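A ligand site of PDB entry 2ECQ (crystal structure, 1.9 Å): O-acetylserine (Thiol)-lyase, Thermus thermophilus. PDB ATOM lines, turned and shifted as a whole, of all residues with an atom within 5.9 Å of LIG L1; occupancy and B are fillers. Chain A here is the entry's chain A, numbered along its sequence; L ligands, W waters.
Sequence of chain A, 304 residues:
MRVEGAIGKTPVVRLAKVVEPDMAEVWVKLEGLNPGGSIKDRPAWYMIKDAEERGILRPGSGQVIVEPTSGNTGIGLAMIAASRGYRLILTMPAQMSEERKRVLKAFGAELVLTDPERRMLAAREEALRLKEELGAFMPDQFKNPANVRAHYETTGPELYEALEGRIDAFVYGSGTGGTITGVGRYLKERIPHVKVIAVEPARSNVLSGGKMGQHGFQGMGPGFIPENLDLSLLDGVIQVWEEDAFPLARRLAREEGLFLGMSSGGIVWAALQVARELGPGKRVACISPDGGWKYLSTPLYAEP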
ATOM      1  N   SER A  38      16.266 -38.280 -10.421  1.00  0.00           N
ATOM      2  CA  SER A  38      16.186 -36.873 -10.050  1.00  0.00           C
ATOM      3  C   SER A  38      15.159 -36.088 -10.848  1.00  0.00           C
ATOM      4  O   SER A  38      14.594 -36.575 -11.835  1.00  0.00           O
ATOM      5  CB  SER A  38      17.541 -36.195 -10.230  1.00  0.00           C
ATOM      6  OG  SER A  38      17.722 -35.810 -11.584  1.00  0.00           O
ATOM      7  N   ILE A  39      14.959 -34.846 -10.422  1.00  0.00           N
ATOM      8  CA  ILE A  39      14.033 -33.934 -11.073  1.00  0.00           C
ATOM      9  C   ILE A  39      14.424 -33.653 -12.527  1.00  0.00           C
ATOM     10  O   ILE A  39      13.566 -33.304 -13.348  1.00  0.00           O
ATOM     11  CB  ILE A  39      13.974 -32.596 -10.291  1.00  0.00           C
ATOM     12  CG1 ILE A  39      12.868 -31.697 -10.853  1.00  0.00           C
ATOM     13  CG2 ILE A  39      15.325 -31.888 -10.369  1.00  0.00           C
ATOM     14  CD1 ILE A  39      12.636 -30.445 -10.015  1.00  0.00           C
ATOM     15  N   LYS A  40      15.708 -33.831 -12.852  1.00  0.00           N
ATOM     16  CA  LYS A  40      16.190 -33.576 -14.207  1.00  0.00           C
ATOM     17  C   LYS A  40      15.603 -34.486 -15.279  1.00  0.00           C
ATOM     18  O   LYS A  40      15.771 -34.221 -16.466  1.00  0.00           O
ATOM     19  CB  LYS A  40      17.716 -33.650 -14.274  1.00  0.00           C
ATOM     20  CG  LYS A  40      18.440 -32.540 -13.552  1.00  0.00           C
ATOM     21  CD  LYS A  40      18.007 -31.160 -14.035  1.00  0.00           C
ATOM     22  CE  LYS A  40      19.114 -30.126 -13.798  1.00  0.00           C
ATOM     23  NZ  LYS A  40      19.602 -30.328 -12.410  1.00  0.00           N
ATOM     24  N   ASN A  72      22.896 -34.511 -12.855  1.00  0.00           N
ATOM     25  CA  ASN A  72      21.601 -35.143 -13.044  1.00  0.00           C
ATOM     26  C   ASN A  72      21.053 -34.971 -14.458  1.00  0.00           C
ATOM     27  O   ASN A  72      20.369 -35.849 -14.967  1.00  0.00           O
ATOM     28  CB  ASN A  72      20.590 -34.614 -12.015  1.00  0.00           C
ATOM     29  CG  ASN A  72      20.800 -35.211 -10.634  1.00  0.00           C
ATOM     30  OD1 ASN A  72      21.101 -36.396 -10.496  1.00  0.00           O
ATOM     31  ND2 ASN A  72      20.637 -34.394  -9.596  1.00  0.00           N
ATOM     32  N   THR A  73      21.344 -33.841 -15.092  1.00  0.00           N
ATOM     33  CA  THR A  73      20.874 -33.619 -16.455  1.00  0.00           C
ATOM     34  C   THR A  73      21.532 -34.643 -17.362  1.00  0.00           C
ATOM     35  O   THR A  73      20.904 -35.188 -18.266  1.00  0.00           O
ATOM     36  CB  THR A  73      21.202 -32.197 -16.937  1.00  0.00           C
ATOM     37  OG1 THR A  73      20.485 -31.250 -16.145  1.00  0.00           O
ATOM     38  CG2 THR A  73      20.797 -32.016 -18.404  1.00  0.00           C
ATOM     39  N   GLN A 141      20.650 -26.831 -21.653  1.00  0.00           N
ATOM     40  CA  GLN A 141      19.795 -26.754 -20.468  1.00  0.00           C
ATOM     41  C   GLN A 141      19.605 -25.425 -19.754  1.00  0.00           C
ATOM     42  O   GLN A 141      18.550 -25.182 -19.178  1.00  0.00           O
ATOM     43  CB  GLN A 141      20.261 -27.795 -19.432  1.00  0.00           C
ATOM     44  CG  GLN A 141      21.552 -27.442 -18.709  1.00  0.00           C
ATOM     45  CD  GLN A 141      21.834 -28.405 -17.567  1.00  0.00           C
ATOM     46  OE1 GLN A 141      20.925 -28.815 -16.850  1.00  0.00           O
ATOM     47  NE2 GLN A 141      23.102 -28.766 -17.396  1.00  0.00           N
ATOM     48  N   ASN A 147      12.862 -26.518 -20.978  1.00  0.00           N
ATOM     49  CA  ASN A 147      13.242 -26.902 -19.618  1.00  0.00           C
ATOM     50  C   ASN A 147      12.164 -26.323 -18.694  1.00  0.00           C
ATOM     51  O   ASN A 147      11.544 -27.049 -17.909  1.00  0.00           O
ATOM     52  CB  ASN A 147      14.612 -26.293 -19.289  1.00  0.00           C
ATOM     53  CG  ASN A 147      15.082 -26.600 -17.863  1.00  0.00           C
ATOM     54  OD1 ASN A 147      14.273 -26.851 -16.973  1.00  0.00           O
ATOM     55  ND2 ASN A 147      16.389 -26.550 -17.655  1.00  0.00           N
ATOM     56  N   HIS A 151       8.342 -28.016 -16.251  1.00  0.00           N
ATOM     57  CA  HIS A 151       7.862 -27.727 -14.907  1.00  0.00           C
ATOM     58  C   HIS A 151       6.546 -26.963 -14.895  1.00  0.00           C
ATOM     59  O   HIS A 151       5.735 -27.105 -13.979  1.00  0.00           O
ATOM     60  CB  HIS A 151       8.955 -26.980 -14.141  1.00  0.00           C
ATOM     61  CG  HIS A 151      10.230 -27.749 -14.041  1.00  0.00           C
ATOM     62  ND1 HIS A 151      10.318 -28.934 -13.335  1.00  0.00           N
ATOM     63  CD2 HIS A 151      11.435 -27.559 -14.611  1.00  0.00           C
ATOM     64  CE1 HIS A 151      11.535 -29.433 -13.485  1.00  0.00           C
ATOM     65  NE2 HIS A 151      12.234 -28.625 -14.261  1.00  0.00           N
ATOM     66  N   TYR A 172      12.802 -23.093  -3.527  1.00  0.00           N
ATOM     67  CA  TYR A 172      13.621 -23.990  -4.340  1.00  0.00           C
ATOM     68  C   TYR A 172      15.054 -23.511  -4.571  1.00  0.00           C
ATOM     69  O   TYR A 172      15.306 -22.320  -4.714  1.00  0.00           O
ATOM     70  CB  TYR A 172      12.959 -24.209  -5.711  1.00  0.00           C
ATOM     71  CG  TYR A 172      13.583 -25.343  -6.496  1.00  0.00           C
ATOM     72  CD1 TYR A 172      13.412 -26.669  -6.092  1.00  0.00           C
ATOM     73  CD2 TYR A 172      14.363 -25.082  -7.623  1.00  0.00           C
ATOM     74  CE1 TYR A 172      14.020 -27.713  -6.784  1.00  0.00           C
ATOM     75  CE2 TYR A 172      14.972 -26.122  -8.325  1.00  0.00           C
ATOM     76  CZ  TYR A 172      14.791 -27.432  -7.905  1.00  0.00           C
ATOM     77  OH  TYR A 172      15.394 -28.476  -8.575  1.00  0.00           O
ATOM     78  N   GLY A 173      15.983 -24.473  -4.603  1.00  0.00           N
ATOM     79  CA  GLY A 173      17.386 -24.162  -4.827  1.00  0.00           C
ATOM     80  C   GLY A 173      17.640 -24.244  -6.319  1.00  0.00           C
ATOM     81  O   GLY A 173      17.743 -25.326  -6.896  1.00  0.00           O
ATOM     82  N   SER A 174      17.750 -23.071  -6.940  1.00  0.00           N
ATOM     83  CA  SER A 174      17.916 -22.961  -8.389  1.00  0.00           C
ATOM     84  C   SER A 174      19.250 -23.400  -8.989  1.00  0.00           C
ATOM     85  O   SER A 174      20.327 -23.090  -8.469  1.00  0.00           O
ATOM     86  CB  SER A 174      17.615 -21.527  -8.829  1.00  0.00           C
ATOM     87  OG  SER A 174      17.474 -21.439 -10.233  1.00  0.00           O
ATOM     88  N   GLY A 175      19.152 -24.116 -10.108  1.00  0.00           N
ATOM     89  CA  GLY A 175      20.314 -24.583 -10.850  1.00  0.00           C
ATOM     90  C   GLY A 175      20.190 -23.919 -12.215  1.00  0.00           C
ATOM     91  O   GLY A 175      20.749 -22.846 -12.432  1.00  0.00           O
ATOM     92  N   THR A 176      19.453 -24.554 -13.130  1.00  0.00           N
ATOM     93  CA  THR A 176      19.240 -24.001 -14.463  1.00  0.00           C
ATOM     94  C   THR A 176      18.156 -22.925 -14.404  1.00  0.00           C
ATOM     95  O   THR A 176      18.042 -22.098 -15.311  1.00  0.00           O
ATOM     96  CB  THR A 176      18.746 -25.063 -15.471  1.00  0.00           C
ATOM     97  OG1 THR A 176      17.462 -25.555 -15.055  1.00  0.00           O
ATOM     98  CG2 THR A 176      19.740 -26.210 -15.584  1.00  0.00           C
ATOM     99  N   GLY A 177      17.372 -22.941 -13.334  1.00  0.00           N
ATOM    100  CA  GLY A 177      16.291 -21.972 -13.187  1.00  0.00           C
ATOM    101  C   GLY A 177      14.968 -22.478 -13.717  1.00  0.00           C
ATOM    102  O   GLY A 177      13.924 -21.867 -13.489  1.00  0.00           O
ATOM    103  N   GLY A 178      14.996 -23.608 -14.423  1.00  0.00           N
ATOM    104  CA  GLY A 178      13.778 -24.155 -14.993  1.00  0.00           C
ATOM    105  C   GLY A 178      12.652 -24.448 -14.014  1.00  0.00           C
ATOM    106  O   GLY A 178      11.498 -24.084 -14.247  1.00  0.00           O
ATOM    107  N   THR A 179      12.984 -25.102 -12.901  1.00  0.00           N
ATOM    108  CA  THR A 179      11.981 -25.462 -11.902  1.00  0.00           C
ATOM    109  C   THR A 179      11.313 -24.272 -11.236  1.00  0.00           C
ATOM    110  O   THR A 179      10.082 -24.180 -11.206  1.00  0.00           O
ATOM    111  CB  THR A 179      12.606 -26.350 -10.805  1.00  0.00           C
ATOM    112  OG1 THR A 179      13.115 -27.551 -11.389  1.00  0.00           O
ATOM    113  CG2 THR A 179      11.571 -26.705  -9.744  1.00  0.00           C
ATOM    114  N   ILE A 180      12.096 -23.359 -10.690  1.00  0.00           N
ATOM    115  CA  ILE A 180      11.511 -22.222 -10.007  1.00  0.00           C
ATOM    116  C   ILE A 180      10.719 -21.320 -10.957  1.00  0.00           C
ATOM    117  O   ILE A 180       9.704 -20.740 -10.567  1.00  0.00           O
ATOM    118  CB  ILE A 180      12.603 -21.408  -9.244  1.00  0.00           C
ATOM    119  CG1 ILE A 180      11.942 -20.532  -8.181  1.00  0.00           C
ATOM    120  CG2 ILE A 180      13.404 -20.554 -10.223  1.00  0.00           C
ATOM    121  CD1 ILE A 180      12.915 -19.989  -7.153  1.00  0.00           C
ATOM    122  N   PHE A 217      26.766 -28.085  -2.714  1.00  0.00           N
ATOM    123  CA  PHE A 217      25.379 -28.422  -3.059  1.00  0.00           C
ATOM    124  C   PHE A 217      25.265 -28.834  -4.527  1.00  0.00           C
ATOM    125  O   PHE A 217      24.760 -28.085  -5.356  1.00  0.00           O
ATOM    126  CB  PHE A 217      24.456 -27.225  -2.796  1.00  0.00           C
ATOM    127  CG  PHE A 217      24.382 -26.805  -1.356  1.00  0.00           C
ATOM    128  CD1 PHE A 217      25.127 -25.723  -0.888  1.00  0.00           C
ATOM    129  CD2 PHE A 217      23.565 -27.478  -0.457  1.00  0.00           C
ATOM    130  CE1 PHE A 217      25.060 -25.320   0.445  1.00  0.00           C
ATOM    131  CE2 PHE A 217      23.485 -27.088   0.879  1.00  0.00           C
ATOM    132  CZ  PHE A 217      24.234 -25.997   1.329  1.00  0.00           C
ATOM    133  N   GLN A 218      25.734 -30.041  -4.831  1.00  0.00           N
ATOM    134  CA  GLN A 218      25.708 -30.529  -6.212  1.00  0.00           C
ATOM    135  C   GLN A 218      24.339 -30.372  -6.867  1.00  0.00           C
ATOM    136  O   GLN A 218      23.309 -30.740  -6.305  1.00  0.00           O
ATOM    137  CB  GLN A 218      26.121 -32.007  -6.259  1.00  0.00           C
ATOM    138  CG  GLN A 218      27.484 -32.278  -5.645  1.00  0.00           C
ATOM    139  CD  GLN A 218      27.969 -33.701  -5.887  1.00  0.00           C
ATOM    140  OE1 GLN A 218      28.801 -34.222  -5.148  1.00  0.00           O
ATOM    141  NE2 GLN A 218      27.462 -34.332  -6.948  1.00  0.00           N
ATOM    142  N   GLY A 219      24.342 -29.795  -8.074  1.00  0.00           N
ATOM    143  CA  GLY A 219      23.102 -29.610  -8.800  1.00  0.00           C
ATOM    144  C   GLY A 219      22.503 -28.218  -8.744  1.00  0.00           C
ATOM    145  O   GLY A 219      21.731 -27.853  -9.629  1.00  0.00           O
ATOM    146  N   MET A 220      22.818 -27.445  -7.718  1.00  0.00           N
ATOM    147  CA  MET A 220      22.288 -26.091  -7.608  1.00  0.00           C
ATOM    148  C   MET A 220      23.408 -25.066  -7.449  1.00  0.00           C
ATOM    149  O   MET A 220      24.545 -25.417  -7.170  1.00  0.00           O
ATOM    150  CB  MET A 220      21.307 -25.963  -6.428  1.00  0.00           C
ATOM    151  CG  MET A 220      21.919 -26.165  -5.047  1.00  0.00           C
ATOM    152  SD  MET A 220      20.721 -25.913  -3.715  1.00  0.00           S
ATOM    153  CE  MET A 220      20.888 -24.159  -3.422  1.00  0.00           C
ATOM    154  N   SER A 263      21.565 -30.897  -2.200  1.00  0.00           N
ATOM    155  CA  SER A 263      20.769 -29.697  -2.478  1.00  0.00           C
ATOM    156  C   SER A 263      19.472 -29.713  -1.682  1.00  0.00           C
ATOM    157  O   SER A 263      18.952 -28.660  -1.302  1.00  0.00           O
ATOM    158  CB  SER A 263      20.466 -29.570  -3.980  1.00  0.00           C
ATOM    159  OG  SER A 263      19.669 -30.646  -4.435  1.00  0.00           O
ATOM    160  N   ILE A 267      17.748 -26.705   0.517  1.00  0.00           N
ATOM    161  CA  ILE A 267      16.405 -26.258   0.189  1.00  0.00           C
ATOM    162  C   ILE A 267      15.447 -26.367   1.379  1.00  0.00           C
ATOM    163  O   ILE A 267      14.695 -25.438   1.661  1.00  0.00           O
ATOM    164  CB  ILE A 267      15.852 -27.058  -1.004  1.00  0.00           C
ATOM    165  CG1 ILE A 267      16.683 -26.729  -2.258  1.00  0.00           C
ATOM    166  CG2 ILE A 267      14.376 -26.737  -1.240  1.00  0.00           C
ATOM    167  CD1 ILE A 267      16.380 -27.594  -3.469  1.00  0.00           C
ATOM    168  N   PRO A 289      15.271 -32.217  -5.071  1.00  0.00           N
ATOM    169  CA  PRO A 289      15.803 -32.571  -6.399  1.00  0.00           C
ATOM    170  C   PRO A 289      16.149 -34.049  -6.585  1.00  0.00           C
ATOM    171  O   PRO A 289      15.849 -34.635  -7.635  1.00  0.00           O
ATOM    172  CB  PRO A 289      17.014 -31.654  -6.538  1.00  0.00           C
ATOM    173  CG  PRO A 289      16.582 -30.443  -5.742  1.00  0.00           C
ATOM    174  CD  PRO A 289      16.024 -31.083  -4.499  1.00  0.00           C
ATOM    175  N   ASP A 290      16.805 -34.654  -5.599  1.00  0.00           N
ATOM    176  CA  ASP A 290      17.152 -36.067  -5.688  1.00  0.00           C
ATOM    177  C   ASP A 290      17.391 -36.708  -4.332  1.00  0.00           C
ATOM    178  O   ASP A 290      17.387 -36.037  -3.301  1.00  0.00           O
ATOM    179  CB  ASP A 290      18.356 -36.297  -6.638  1.00  0.00           C
ATOM    180  CG  ASP A 290      19.646 -35.630  -6.166  1.00  0.00           C
ATOM    181  OD1 ASP A 290      20.666 -35.782  -6.888  1.00  0.00           O
ATOM    182  OD2 ASP A 290      19.668 -34.961  -5.108  1.00  0.00           O
ATOM    183  N   TYR A 295      25.197 -39.958  -3.170  1.00  0.00           N
ATOM    184  CA  TYR A 295      26.131 -39.230  -2.326  1.00  0.00           C
ATOM    185  C   TYR A 295      26.692 -39.935  -1.094  1.00  0.00           C
ATOM    186  O   TYR A 295      27.076 -39.271  -0.123  1.00  0.00           O
ATOM    187  CB  TYR A 295      25.470 -37.916  -1.905  1.00  0.00           C
ATOM    188  CG  TYR A 295      24.816 -37.198  -3.063  1.00  0.00           C
ATOM    189  CD1 TYR A 295      23.434 -37.303  -3.291  1.00  0.00           C
ATOM    190  CD2 TYR A 295      25.570 -36.432  -3.946  1.00  0.00           C
ATOM    191  CE1 TYR A 295      22.829 -36.665  -4.373  1.00  0.00           C
ATOM    192  CE2 TYR A 295      24.976 -35.791  -5.036  1.00  0.00           C
ATOM    193  CZ  TYR A 295      23.610 -35.906  -5.242  1.00  0.00           C
ATOM    194  OH  TYR A 295      23.035 -35.253  -6.311  1.00  0.00           O
HETATM  195  N1  LIG L   1      19.551 -29.762  -7.190  1.00  0.00           N
HETATM  196  C1  LIG L   1      19.953 -30.825  -7.948  1.00  0.00           C
HETATM  197  C2  LIG L   1      20.600 -32.040  -7.241  1.00  0.00           C
HETATM  198  C3  LIG L   1      19.771 -30.799  -9.334  1.00  0.00           C
HETATM  199  O1  LIG L   1      20.185 -31.859 -10.100  1.00  0.00           O
HETATM  200  C4  LIG L   1      19.185 -29.692  -9.931  1.00  0.00           C
HETATM  201  C5  LIG L   1      18.956 -29.641 -11.440  1.00  0.00           C
HETATM  202  C6  LIG L   1      18.768 -28.604  -9.131  1.00  0.00           C
HETATM  203  C7  LIG L   1      18.960 -28.663  -7.769  1.00  0.00           C
HETATM  204  C8  LIG L   1      18.096 -27.323  -9.714  1.00  0.00           C
HETATM  205  O2  LIG L   1      16.877 -27.467 -10.539  1.00  0.00           O
HETATM  206  P1  LIG L   1      16.779 -26.493 -11.790  1.00  0.00           P
HETATM  207  O3  LIG L   1      17.810 -26.883 -12.786  1.00  0.00           O
HETATM  208  O4  LIG L   1      15.370 -26.663 -12.424  1.00  0.00           O
HETATM  209  O5  LIG L   1      16.836 -25.129 -11.240  1.00  0.00           O
HETATM  210  C1  LG2 L   2      22.555 -29.370 -14.342  1.00  0.00           C
HETATM  211  C2  LG2 L   2      22.971 -28.152 -13.427  1.00  0.00           C
HETATM  212  O1  LG2 L   2      21.989 -27.910 -12.399  1.00  0.00           O
HETATM  213  C3  LG2 L   2      24.347 -28.377 -12.745  1.00  0.00           C
HETATM  214  C4  LG2 L   2      22.920 -30.826 -13.930  1.00  0.00           C
HETATM  215  O2  LG2 L   2      22.186 -31.356 -13.060  1.00  0.00           O
HETATM  216  O3  LG2 L   2      23.890 -31.395 -14.460  1.00  0.00           O
HETATM  217  O   HOH W   1      23.077 -32.552 -10.830  1.00  0.00           O
HETATM  218  O   HOH W   2      22.529 -32.459  -4.379  1.00  0.00           O
HETATM  219  O   HOH W   3      14.883 -28.192 -14.694  1.00  0.00           O
HETATM  220  O   HOH W   4      15.110 -23.376 -10.527  1.00  0.00           O
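The backbone NH (N) of Lys 40 lies close to the side-chain hydroxyl (OG) of Ser 38 (3.1 Å). The side-chain amide nitrogen (ND2) of Asn 72 is in hydrogen-bond range of the side-chain carboxylate (OD1) of Asp 290 (3.0 Å). A ring nitrogen (NE2) of His 151 lies within hydrogen-bond range of the side-chain hydroxyl of Thr 179, 3.2 Å away. The side-chain hydroxyl (OG1) of Thr 176 lies within hydrogen-bond range of the backbone NH (N) of Gly 178 (3.2 Å). The side-chain hydroxyl of Thr 176 lies within hydrogen-bond range of the side-chain amide nitrogen of Asn 147. The backbone NH (N) of Gly 177 sits close to the side-chain hydroxyl (OG) of Ser 174, 3.4 Å away. N of Ile 39 is in hydrogen-bond range of O of Pro 289, at 2.9 Å. The side-chain carboxylate (OD1) of Asp 290 is in hydrogen-bond range of the side-chain hydroxyl (OH) of Tyr 295 (2.5 Å).
Water W4 lies within hydrogen-bond range of an oxygen (O5) of LIG L1 (2.6 Å), the backbone NH of Ile 180 (3.0 Å) and the side-chain hydroxyl of Ser 174 (3.1 Å). Water W3 lies within hydrogen-bond range of the side-chain amide oxygen of Asn 147 (2.7 Å), a ring nitrogen (NE2) of His 151 (2.7 Å) and an oxygen (O4) of LIG L1 (2.8 Å). Water W1 lies within hydrogen-bond range of O2 of LG2 L2, N of Asn 72 and O1 of LIG L1. Water W2 lies within hydrogen-bond range of O of Gln 218 (2.7 Å), N of Ser 263 (2.8 Å) and OH of Tyr 295 (3.4 Å).
C5 of LIG L1 is covalently linked to NZ of Lys 40 (1.4 Å). O1 of LIG L1 is in hydrogen-bond range of ND2 of Asn 72 (2.6 Å). An oxygen (O4) of LIG L1 sits at hydrogen-bond distance from the backbone NH (N) of Thr 179, at 2.9 Å. OG1 of Thr 179 is in hydrogen-bond range of O4 of LIG L1, 2.6 Å away. The backbone NH (N) of Thr 176 sits at hydrogen-bond distance from an oxygen (O3) of LIG L1 (2.9 Å). The side-chain hydroxyl (OG1) of Thr 176 lies within hydrogen-bond range of an oxygen (O3) of LIG L1 (2.7 Å). The side-chain hydroxyl (OH) of Tyr 172 is in hydrogen-bond range of an oxygen (O2) of LIG L1 (2.7 Å). The backbone NH (N) of Gly 175 lies within hydrogen-bond range of an oxygen (O5) of LIG L1, at 2.8 Å. A nitrogen (N1) of LIG L1 sits at hydrogen-bond distance from the side-chain hydroxyl (OG) of Ser 263, 2.9 Å away. O5 of LIG L1 sits at hydrogen-bond distance from N of Gly 177 (3.1 Å). An oxygen (O2) of LG2 L2 lies within salt-bridge range of the side-chain amino group (NZ) of Lys 40. O2 of LG2 L2 lies within hydrogen-bond range of N of Asn 72. The backbone carbonyl oxygen of Gly 219 is in hydrogen-bond range of an oxygen (O1) of LG2 L2, at 2.8 Å. The backbone NH of Thr 73 sits at hydrogen-bond distance from an oxygen (O2) of LG2 L2 (3.3 Å).
Gly 173 touches LIG L1. Ser 174 touches LIG L1 (C to O5, 3.7 Å). Gly 178 touches LIG L1. O of Gln 218 touches C2 of LIG L1, at 3.1 Å. Gly 219 touches LIG L1. Met 220 touches LIG L1. Pro 289 touches LIG L1 (CB to N1, 3.2 Å). Asp 290 touches LIG L1 (OD2 to C2, 3.7 Å). Hydrophobic or aromatic side chains within 4 Å of LIG L1: Tyr 172, Met 220 and Pro 289. 16 residues have an atom within 4 Å of LIG L1: Lys 40, Asn 72, Tyr 172, Gly 173, Ser 174, Gly 175, Thr 176, Gly 177, Gly 178, Thr 179, Gln 218, Gly 219, Met 220, Ser 263, Pro 289 and Asp 290. The nearest printed residue that does not touch LIG L1 is His 151 (4.1 Å).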
